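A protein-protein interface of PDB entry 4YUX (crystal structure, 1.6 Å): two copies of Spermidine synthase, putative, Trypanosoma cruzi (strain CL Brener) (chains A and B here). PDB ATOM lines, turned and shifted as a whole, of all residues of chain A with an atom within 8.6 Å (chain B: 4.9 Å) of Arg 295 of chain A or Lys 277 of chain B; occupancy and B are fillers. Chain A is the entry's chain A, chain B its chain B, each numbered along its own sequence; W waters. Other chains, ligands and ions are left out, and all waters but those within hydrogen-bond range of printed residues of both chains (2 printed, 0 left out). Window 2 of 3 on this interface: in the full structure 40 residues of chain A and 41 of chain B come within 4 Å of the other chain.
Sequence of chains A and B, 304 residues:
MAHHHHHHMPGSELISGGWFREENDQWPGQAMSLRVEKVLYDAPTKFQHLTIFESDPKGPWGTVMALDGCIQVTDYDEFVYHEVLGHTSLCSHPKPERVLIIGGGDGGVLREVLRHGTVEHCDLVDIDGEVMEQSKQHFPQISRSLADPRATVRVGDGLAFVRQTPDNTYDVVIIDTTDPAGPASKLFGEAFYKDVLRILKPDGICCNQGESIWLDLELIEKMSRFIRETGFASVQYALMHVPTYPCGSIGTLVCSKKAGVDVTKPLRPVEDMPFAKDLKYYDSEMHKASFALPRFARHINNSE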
ATOM      1  N   ILE A 213      14.157   5.785  10.223  1.00  0.00           N
ATOM      2  CA  ILE A 213      14.243   5.684  11.723  1.00  0.00           C
ATOM      3  C   ILE A 213      12.881   5.926  12.402  1.00  0.00           C
ATOM      4  O   ILE A 213      12.754   5.623  13.579  1.00  0.00           O
ATOM      5  CB  ILE A 213      15.308   6.641  12.323  1.00  0.00           C
ATOM      6  CG1 ILE A 213      14.989   8.074  11.978  1.00  0.00           C
ATOM      7  CG2 ILE A 213      16.713   6.082  11.910  1.00  0.00           C
ATOM      8  CD1 ILE A 213      15.916   9.111  12.682  1.00  0.00           C
ATOM      9  N   LEU A 217      12.644   1.341  12.885  1.00  0.00           N
ATOM     10  CA  LEU A 217      13.766   1.294  13.768  1.00  0.00           C
ATOM     11  C   LEU A 217      14.104  -0.086  14.263  1.00  0.00           C
ATOM     12  O   LEU A 217      15.287  -0.425  14.390  1.00  0.00           O
ATOM     13  CB  LEU A 217      13.583   2.255  14.972  1.00  0.00           C
ATOM     14  CG  LEU A 217      14.850   2.515  15.815  1.00  0.00           C
ATOM     15  CD1 LEU A 217      15.971   3.148  14.963  1.00  0.00           C
ATOM     16  CD2 LEU A 217      14.462   3.477  16.982  1.00  0.00           C
ATOM     17  N   ALA A 292      25.291  11.891  12.698  1.00  0.00           N
ATOM     18  CA  ALA A 292      24.688  12.324  13.958  1.00  0.00           C
ATOM     19  C   ALA A 292      23.231  11.944  13.971  1.00  0.00           C
ATOM     20  O   ALA A 292      22.484  12.353  13.026  1.00  0.00           O
ATOM     21  CB  ALA A 292      24.873  13.780  14.097  1.00  0.00           C
ATOM     22  N   LEU A 293      22.773  11.133  14.949  1.00  0.00           N
ATOM     23  CA  LEU A 293      21.417  10.599  14.928  1.00  0.00           C
ATOM     24  C   LEU A 293      20.609  11.226  16.100  1.00  0.00           C
ATOM     25  O   LEU A 293      21.194  11.577  17.124  1.00  0.00           O
ATOM     26  CB  LEU A 293      21.375   9.060  15.064  1.00  0.00           C
ATOM     27  CG  LEU A 293      22.234   8.391  13.948  1.00  0.00           C
ATOM     28  CD1 LEU A 293      21.916   6.938  14.185  1.00  0.00           C
ATOM     29  CD2 LEU A 293      21.611   8.794  12.603  1.00  0.00           C
ATOM     30  N   PRO A 294      19.354  11.434  15.891  1.00  0.00           N
ATOM     31  CA  PRO A 294      18.526  11.905  17.021  1.00  0.00           C
ATOM     32  C   PRO A 294      18.686  10.941  18.217  1.00  0.00           C
ATOM     33  O   PRO A 294      18.948   9.727  18.072  1.00  0.00           O
ATOM     34  CB  PRO A 294      17.119  11.717  16.493  1.00  0.00           C
ATOM     35  CG  PRO A 294      17.223  11.812  14.996  1.00  0.00           C
ATOM     36  CD  PRO A 294      18.531  11.186  14.681  1.00  0.00           C
ATOM     37  N   ARG A 295      18.569  11.480  19.412  1.00  0.00           N
ATOM     38  CA  ARG A 295      18.816  10.660  20.603  1.00  0.00           C
ATOM     39  C   ARG A 295      18.006   9.373  20.582  1.00  0.00           C
ATOM     40  O   ARG A 295      18.543   8.339  21.016  1.00  0.00           O
ATOM     41  CB  ARG A 295      18.469  11.504  21.849  1.00  0.00           C
ATOM     42  CG  ARG A 295      19.705  12.227  22.259  1.00  0.00           C
ATOM     43  CD  ARG A 295      19.574  12.950  23.617  1.00  0.00           C
ATOM     44  NE  ARG A 295      18.958  12.112  24.616  1.00  0.00           N
ATOM     45  CZ  ARG A 295      19.592  11.254  25.371  1.00  0.00           C
ATOM     46  NH1 ARG A 295      20.914  11.062  25.216  1.00  0.00           N
ATOM     47  NH2 ARG A 295      18.874  10.510  26.166  1.00  0.00           N
ATOM     48  N   PHE A 296      16.738   9.361  20.156  1.00  0.00           N
ATOM     49  CA  PHE A 296      15.940   8.107  20.155  1.00  0.00           C
ATOM     50  C   PHE A 296      16.590   6.994  19.327  1.00  0.00           C
ATOM     51  O   PHE A 296      16.227   5.790  19.477  1.00  0.00           O
ATOM     52  CB  PHE A 296      14.494   8.364  19.817  1.00  0.00           C
ATOM     53  CG  PHE A 296      14.192   8.710  18.368  1.00  0.00           C
ATOM     54  CD1 PHE A 296      13.996   7.675  17.419  1.00  0.00           C
ATOM     55  CD2 PHE A 296      14.022  10.006  17.925  1.00  0.00           C
ATOM     56  CE1 PHE A 296      13.716   7.965  16.111  1.00  0.00           C
ATOM     57  CE2 PHE A 296      13.732  10.305  16.560  1.00  0.00           C
ATOM     58  CZ  PHE A 296      13.568   9.261  15.632  1.00  0.00           C
ATOM     59  N   ALA A 297      17.353   7.431  18.326  1.00  0.00           N
ATOM     60  CA  ALA A 297      17.965   6.406  17.423  1.00  0.00           C
ATOM     61  C   ALA A 297      19.454   6.208  17.616  1.00  0.00           C
ATOM     62  O   ALA A 297      20.068   5.446  16.872  1.00  0.00           O
ATOM     63  CB  ALA A 297      17.675   6.843  15.985  1.00  0.00           C
ATOM     64  N   ARG A 298      20.122   6.916  18.565  1.00  0.00           N
ATOM     65  CA  ARG A 298      21.635   7.067  18.540  1.00  0.00           C
ATOM     66  C   ARG A 298      22.320   5.744  18.841  1.00  0.00           C
ATOM     67  O   ARG A 298      23.462   5.575  18.480  1.00  0.00           O
ATOM     68  CB  ARG A 298      22.154   8.141  19.524  1.00  0.00           C
ATOM     69  CG  ARG A 298      21.826   7.715  20.950  1.00  0.00           C
ATOM     70  CD  ARG A 298      22.215   8.656  22.076  1.00  0.00           C
ATOM     71  NE  ARG A 298      22.122   7.888  23.340  1.00  0.00           N
ATOM     72  CZ  ARG A 298      20.998   7.678  24.034  1.00  0.00           C
ATOM     73  NH1 ARG A 298      19.843   8.158  23.625  1.00  0.00           N
ATOM     74  NH2 ARG A 298      21.003   6.979  25.170  1.00  0.00           N
ATOM     75  N   HIS A 299      21.577   4.803  19.456  1.00  0.00           N
ATOM     76  CA  HIS A 299      22.185   3.572  19.857  1.00  0.00           C
ATOM     77  C   HIS A 299      22.552   2.762  18.642  1.00  0.00           C
ATOM     78  O   HIS A 299      23.448   1.963  18.742  1.00  0.00           O
ATOM     79  CB  HIS A 299      21.234   2.692  20.700  1.00  0.00           C
ATOM     80  CG  HIS A 299      19.904   2.479  20.090  1.00  0.00           C
ATOM     81  ND1 HIS A 299      18.953   3.492  20.051  1.00  0.00           N
ATOM     82  CD2 HIS A 299      19.325   1.405  19.524  1.00  0.00           C
ATOM     83  CE1 HIS A 299      17.837   3.029  19.509  1.00  0.00           C
ATOM     84  NE2 HIS A 299      18.062   1.760  19.133  1.00  0.00           N
ATOM     85  N   ILE A 300      21.946   3.024  17.448  1.00  0.00           N
ATOM     86  CA  ILE A 300      22.392   2.326  16.264  1.00  0.00           C
ATOM     87  C   ILE A 300      23.912   2.636  16.077  1.00  0.00           C
ATOM     88  O   ILE A 300      24.638   1.790  15.602  1.00  0.00           O
ATOM     89  CB  ILE A 300      21.615   2.881  14.977  1.00  0.00           C
ATOM     90  CG1 ILE A 300      20.097   2.724  15.144  1.00  0.00           C
ATOM     91  CG2 ILE A 300      22.165   2.266  13.658  1.00  0.00           C
ATOM     92  CD1 ILE A 300      19.674   1.334  15.580  1.00  0.00           C
ATOM     93  N   PRO B 274      21.301  19.066  33.715  1.00  0.00           N
ATOM     94  CA  PRO B 274      20.657  17.852  34.236  1.00  0.00           C
ATOM     95  C   PRO B 274      19.585  17.144  33.434  1.00  0.00           C
ATOM     96  O   PRO B 274      19.286  15.947  33.666  1.00  0.00           O
ATOM     97  CB  PRO B 274      20.045  18.320  35.597  1.00  0.00           C
ATOM     98  CG  PRO B 274      20.145  19.774  35.611  1.00  0.00           C
ATOM     99  CD  PRO B 274      20.982  20.284  34.504  1.00  0.00           C
ATOM    100  N   PHE B 275      19.025  17.847  32.442  1.00  0.00           N
ATOM    101  CA  PHE B 275      17.922  17.266  31.687  1.00  0.00           C
ATOM    102  C   PHE B 275      18.365  16.731  30.318  1.00  0.00           C
ATOM    103  O   PHE B 275      17.504  16.297  29.574  1.00  0.00           O
ATOM    104  CB  PHE B 275      16.836  18.371  31.470  1.00  0.00           C
ATOM    105  CG  PHE B 275      17.364  19.610  30.738  1.00  0.00           C
ATOM    106  CD1 PHE B 275      17.338  19.609  29.332  1.00  0.00           C
ATOM    107  CD2 PHE B 275      17.860  20.733  31.435  1.00  0.00           C
ATOM    108  CE1 PHE B 275      17.860  20.720  28.637  1.00  0.00           C
ATOM    109  CE2 PHE B 275      18.341  21.819  30.762  1.00  0.00           C
ATOM    110  CZ  PHE B 275      18.315  21.827  29.351  1.00  0.00           C
ATOM    111  N   ALA B 276      19.688  16.730  30.014  1.00  0.00           N
ATOM    112  CA  ALA B 276      20.088  16.253  28.632  1.00  0.00           C
ATOM    113  C   ALA B 276      19.535  14.869  28.355  1.00  0.00           C
ATOM    114  O   ALA B 276      19.141  14.570  27.238  1.00  0.00           O
ATOM    115  CB  ALA B 276      21.608  16.230  28.525  1.00  0.00           C
ATOM    116  N   LYS B 277      19.537  14.002  29.365  1.00  0.00           N
ATOM    117  CA  LYS B 277      19.007  12.649  29.136  1.00  0.00           C
ATOM    118  C   LYS B 277      17.535  12.480  28.955  1.00  0.00           C
ATOM    119  O   LYS B 277      17.107  11.413  28.524  1.00  0.00           O
ATOM    120  CB  LYS B 277      19.557  11.741  30.259  1.00  0.00           C
ATOM    121  CG  LYS B 277      21.077  11.653  30.049  1.00  0.00           C
ATOM    122  CD  LYS B 277      21.766  11.149  31.316  1.00  0.00           C
ATOM    123  CE  LYS B 277      23.267  10.941  31.085  1.00  0.00           C
ATOM    124  NZ  LYS B 277      23.891  10.004  32.070  1.00  0.00           N
ATOM    125  N   ASP B 278      16.721  13.511  29.220  1.00  0.00           N
ATOM    126  CA  ASP B 278      15.317  13.439  29.020  1.00  0.00           C
ATOM    127  C   ASP B 278      14.945  13.774  27.535  1.00  0.00           C
ATOM    128  O   ASP B 278      13.751  13.609  27.131  1.00  0.00           O
ATOM    129  CB  ASP B 278      14.634  14.470  29.900  1.00  0.00           C
ATOM    130  CG  ASP B 278      14.900  14.264  31.370  1.00  0.00           C
ATOM    131  OD1 ASP B 278      15.003  13.068  31.723  1.00  0.00           O
ATOM    132  OD2 ASP B 278      14.946  15.298  32.107  1.00  0.00           O
ATOM    133  N   LEU B 279      15.905  14.299  26.793  1.00  0.00           N
ATOM    134  CA  LEU B 279      15.528  14.759  25.419  1.00  0.00           C
ATOM    135  C   LEU B 279      15.443  13.559  24.481  1.00  0.00           C
ATOM    136  O   LEU B 279      16.293  12.633  24.599  1.00  0.00           O
ATOM    137  CB  LEU B 279      16.579  15.789  24.889  1.00  0.00           C
ATOM    138  CG  LEU B 279      16.662  17.021  25.818  1.00  0.00           C
ATOM    139  CD1 LEU B 279      17.599  18.095  25.223  1.00  0.00           C
ATOM    140  CD2 LEU B 279      15.355  17.696  26.236  1.00  0.00           C
ATOM    141  N   LYS B 280      14.599  13.684  23.430  1.00  0.00           N
ATOM    142  CA  LYS B 280      14.414  12.556  22.492  1.00  0.00           C
ATOM    143  C   LYS B 280      15.067  12.789  21.128  1.00  0.00           C
ATOM    144  O   LYS B 280      15.221  11.827  20.347  1.00  0.00           O
ATOM    145  CB  LYS B 280      12.951  12.313  22.326  1.00  0.00           C
ATOM    146  CG  LYS B 280      12.245  11.809  23.604  1.00  0.00           C
ATOM    147  CD  LYS B 280      10.682  12.059  23.450  1.00  0.00           C
ATOM    148  CE  LYS B 280       9.821  11.291  24.452  1.00  0.00           C
ATOM    149  NZ  LYS B 280       9.642  11.955  25.779  1.00  0.00           N
ATOM    150  N   TYR B 281      15.472  14.029  20.855  1.00  0.00           N
ATOM    151  CA  TYR B 281      16.138  14.346  19.602  1.00  0.00           C
ATOM    152  C   TYR B 281      17.451  15.047  19.793  1.00  0.00           C
ATOM    153  O   TYR B 281      18.535  14.597  19.315  1.00  0.00           O
ATOM    154  CB  TYR B 281      15.182  15.301  18.750  1.00  0.00           C
ATOM    155  CG  TYR B 281      15.638  15.621  17.333  1.00  0.00           C
ATOM    156  CD1 TYR B 281      15.256  14.799  16.270  1.00  0.00           C
ATOM    157  CD2 TYR B 281      16.426  16.713  17.049  1.00  0.00           C
ATOM    158  CE1 TYR B 281      15.614  15.119  14.942  1.00  0.00           C
ATOM    159  CE2 TYR B 281      16.802  17.009  15.768  1.00  0.00           C
ATOM    160  CZ  TYR B 281      16.407  16.198  14.711  1.00  0.00           C
ATOM    161  OH  TYR B 281      16.776  16.540  13.396  1.00  0.00           O
ATOM    162  N   TYR B 282      17.417  16.188  20.439  1.00  0.00           N
ATOM    163  CA  TYR B 282      18.554  17.080  20.491  1.00  0.00           C
ATOM    164  C   TYR B 282      19.668  16.677  21.488  1.00  0.00           C
ATOM    165  O   TYR B 282      19.410  16.194  22.606  1.00  0.00           O
ATOM    166  CB  TYR B 282      18.027  18.485  20.964  1.00  0.00           C
ATOM    167  CG  TYR B 282      19.090  19.534  21.118  1.00  0.00           C
ATOM    168  CD1 TYR B 282      19.777  19.728  22.370  1.00  0.00           C
ATOM    169  CD2 TYR B 282      19.439  20.452  20.082  1.00  0.00           C
ATOM    170  CE1 TYR B 282      20.823  20.644  22.474  1.00  0.00           C
ATOM    171  CE2 TYR B 282      20.444  21.425  20.219  1.00  0.00           C
ATOM    172  CZ  TYR B 282      21.181  21.488  21.428  1.00  0.00           C
ATOM    173  OH  TYR B 282      22.134  22.437  21.650  1.00  0.00           O
ATOM    174  N   ASP B 283      20.867  16.886  20.991  1.00  0.00           N
ATOM    175  CA  ASP B 283      22.112  16.824  21.812  1.00  0.00           C
ATOM    176  C   ASP B 283      23.147  17.681  21.106  1.00  0.00           C
ATOM    177  O   ASP B 283      22.877  18.269  20.015  1.00  0.00           O
ATOM    178  CB  ASP B 283      22.541  15.376  22.135  1.00  0.00           C
ATOM    179  CG  ASP B 283      22.968  14.582  20.909  1.00  0.00           C
ATOM    180  OD1 ASP B 283      23.257  15.135  19.805  1.00  0.00           O
ATOM    181  OD2 ASP B 283      23.013  13.306  20.986  1.00  0.00           O
HETATM  182  O   HOH W   1      23.103  12.380  23.620  1.00  0.00           O
HETATM  183  O   HOH W   2      22.220  11.078  19.787  1.00  0.00           O
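Of the 10 printed residues of chain B, 7 touch a printed residue of chain A. Printed residues of chain B that touch a printed residue of chain A: Ala 276, Lys 277, Leu 279, Lys 280, Tyr 281, Tyr 282 and Asp 283. Hydrophobic or aromatic side chains of chain B that line the printed part of chain A: Tyr 281. Of the 11 printed residues of chain A, 3 touch a printed residue of chain B. Printed residues of chain A that touch a printed residue of chain B: Pro 294, Arg 295 and Phe 296. Hydrophobic or aromatic side chains of chain A within 4 Å of the printed part of chain B: Pro 294 and Phe 296. Among the printed residues, no Asp or Glu carboxylate lies within 4 Å of a Lys or Arg side-chain nitrogen of the other chain.
Water W2 lies within hydrogen-bond range of the side-chain carboxylate of Asp 283 of chain B (2.7 Å) and the backbone carbonyl oxygen of Leu 293 of chain A (2.9 Å). Water W1 bridges OD2 of Asp 283 of chain B (2.8 Å) and NH1 of Arg 295 of chain A (3.0 Å).
The backbone carbonyl oxygen (O) of Arg 295 of chain A lies within hydrogen-bond range of the guanidinium group (NH1) of Arg 298 of chain A (2.9 Å).
No position is printed for both chains.
Of the printed residues of chain B, Pro 294 of chain A touches Tyr 281 (3.5 Å). Of chain B, only Ala 276 (3.6 Å), Lys 277 (3.1 Å), Leu 279 (2.7 Å), Lys 280 (3.5 Å), Tyr 281 (3.1 Å), Tyr 282 (3.4 Å) and Asp 283 (3.7 Å) come within 4 Å of Arg 295 of chain A. Lys 277 of chain B touches one residue of chain A. Of the printed residues of chain A, Leu 279 of chain B touches Arg 295. The nearest residue of chain A that does not touch Lys 277 of chain B is Arg 298 of chain A (6.5 Å).
Among the printed residues, pairs that only touch across the chains: Pro 294 of chain A with Tyr 281 of chain B, Arg 295 of chain A with Ala 276 of chain B, Arg 295 of chain A with Tyr 282 of chain B and Arg 295 of chain A with Asp 283 of chain B.
The guanidinium group of Arg 295 of chain A is in hydrogen-bond range of the backbone carbonyl oxygen of Lys 277 of chain B (3.1 Å). N of Phe 296 of chain A sits at hydrogen-bond distance from O of Lys 280 of chain B. O of Tyr 281 of chain B lies within hydrogen-bond range of N of Arg 295 of chain A (3.1 Å). The guanidinium group (NE) of Arg 295 of chain A sits at hydrogen-bond distance from the backbone carbonyl oxygen (O) of Leu 279 of chain B (2.7 Å). The backbone NH (N) of Arg 295 of chain A is in hydrogen-bond range of the backbone carbonyl oxygen (O) of Lys 280 of chain B (3.5 Å).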
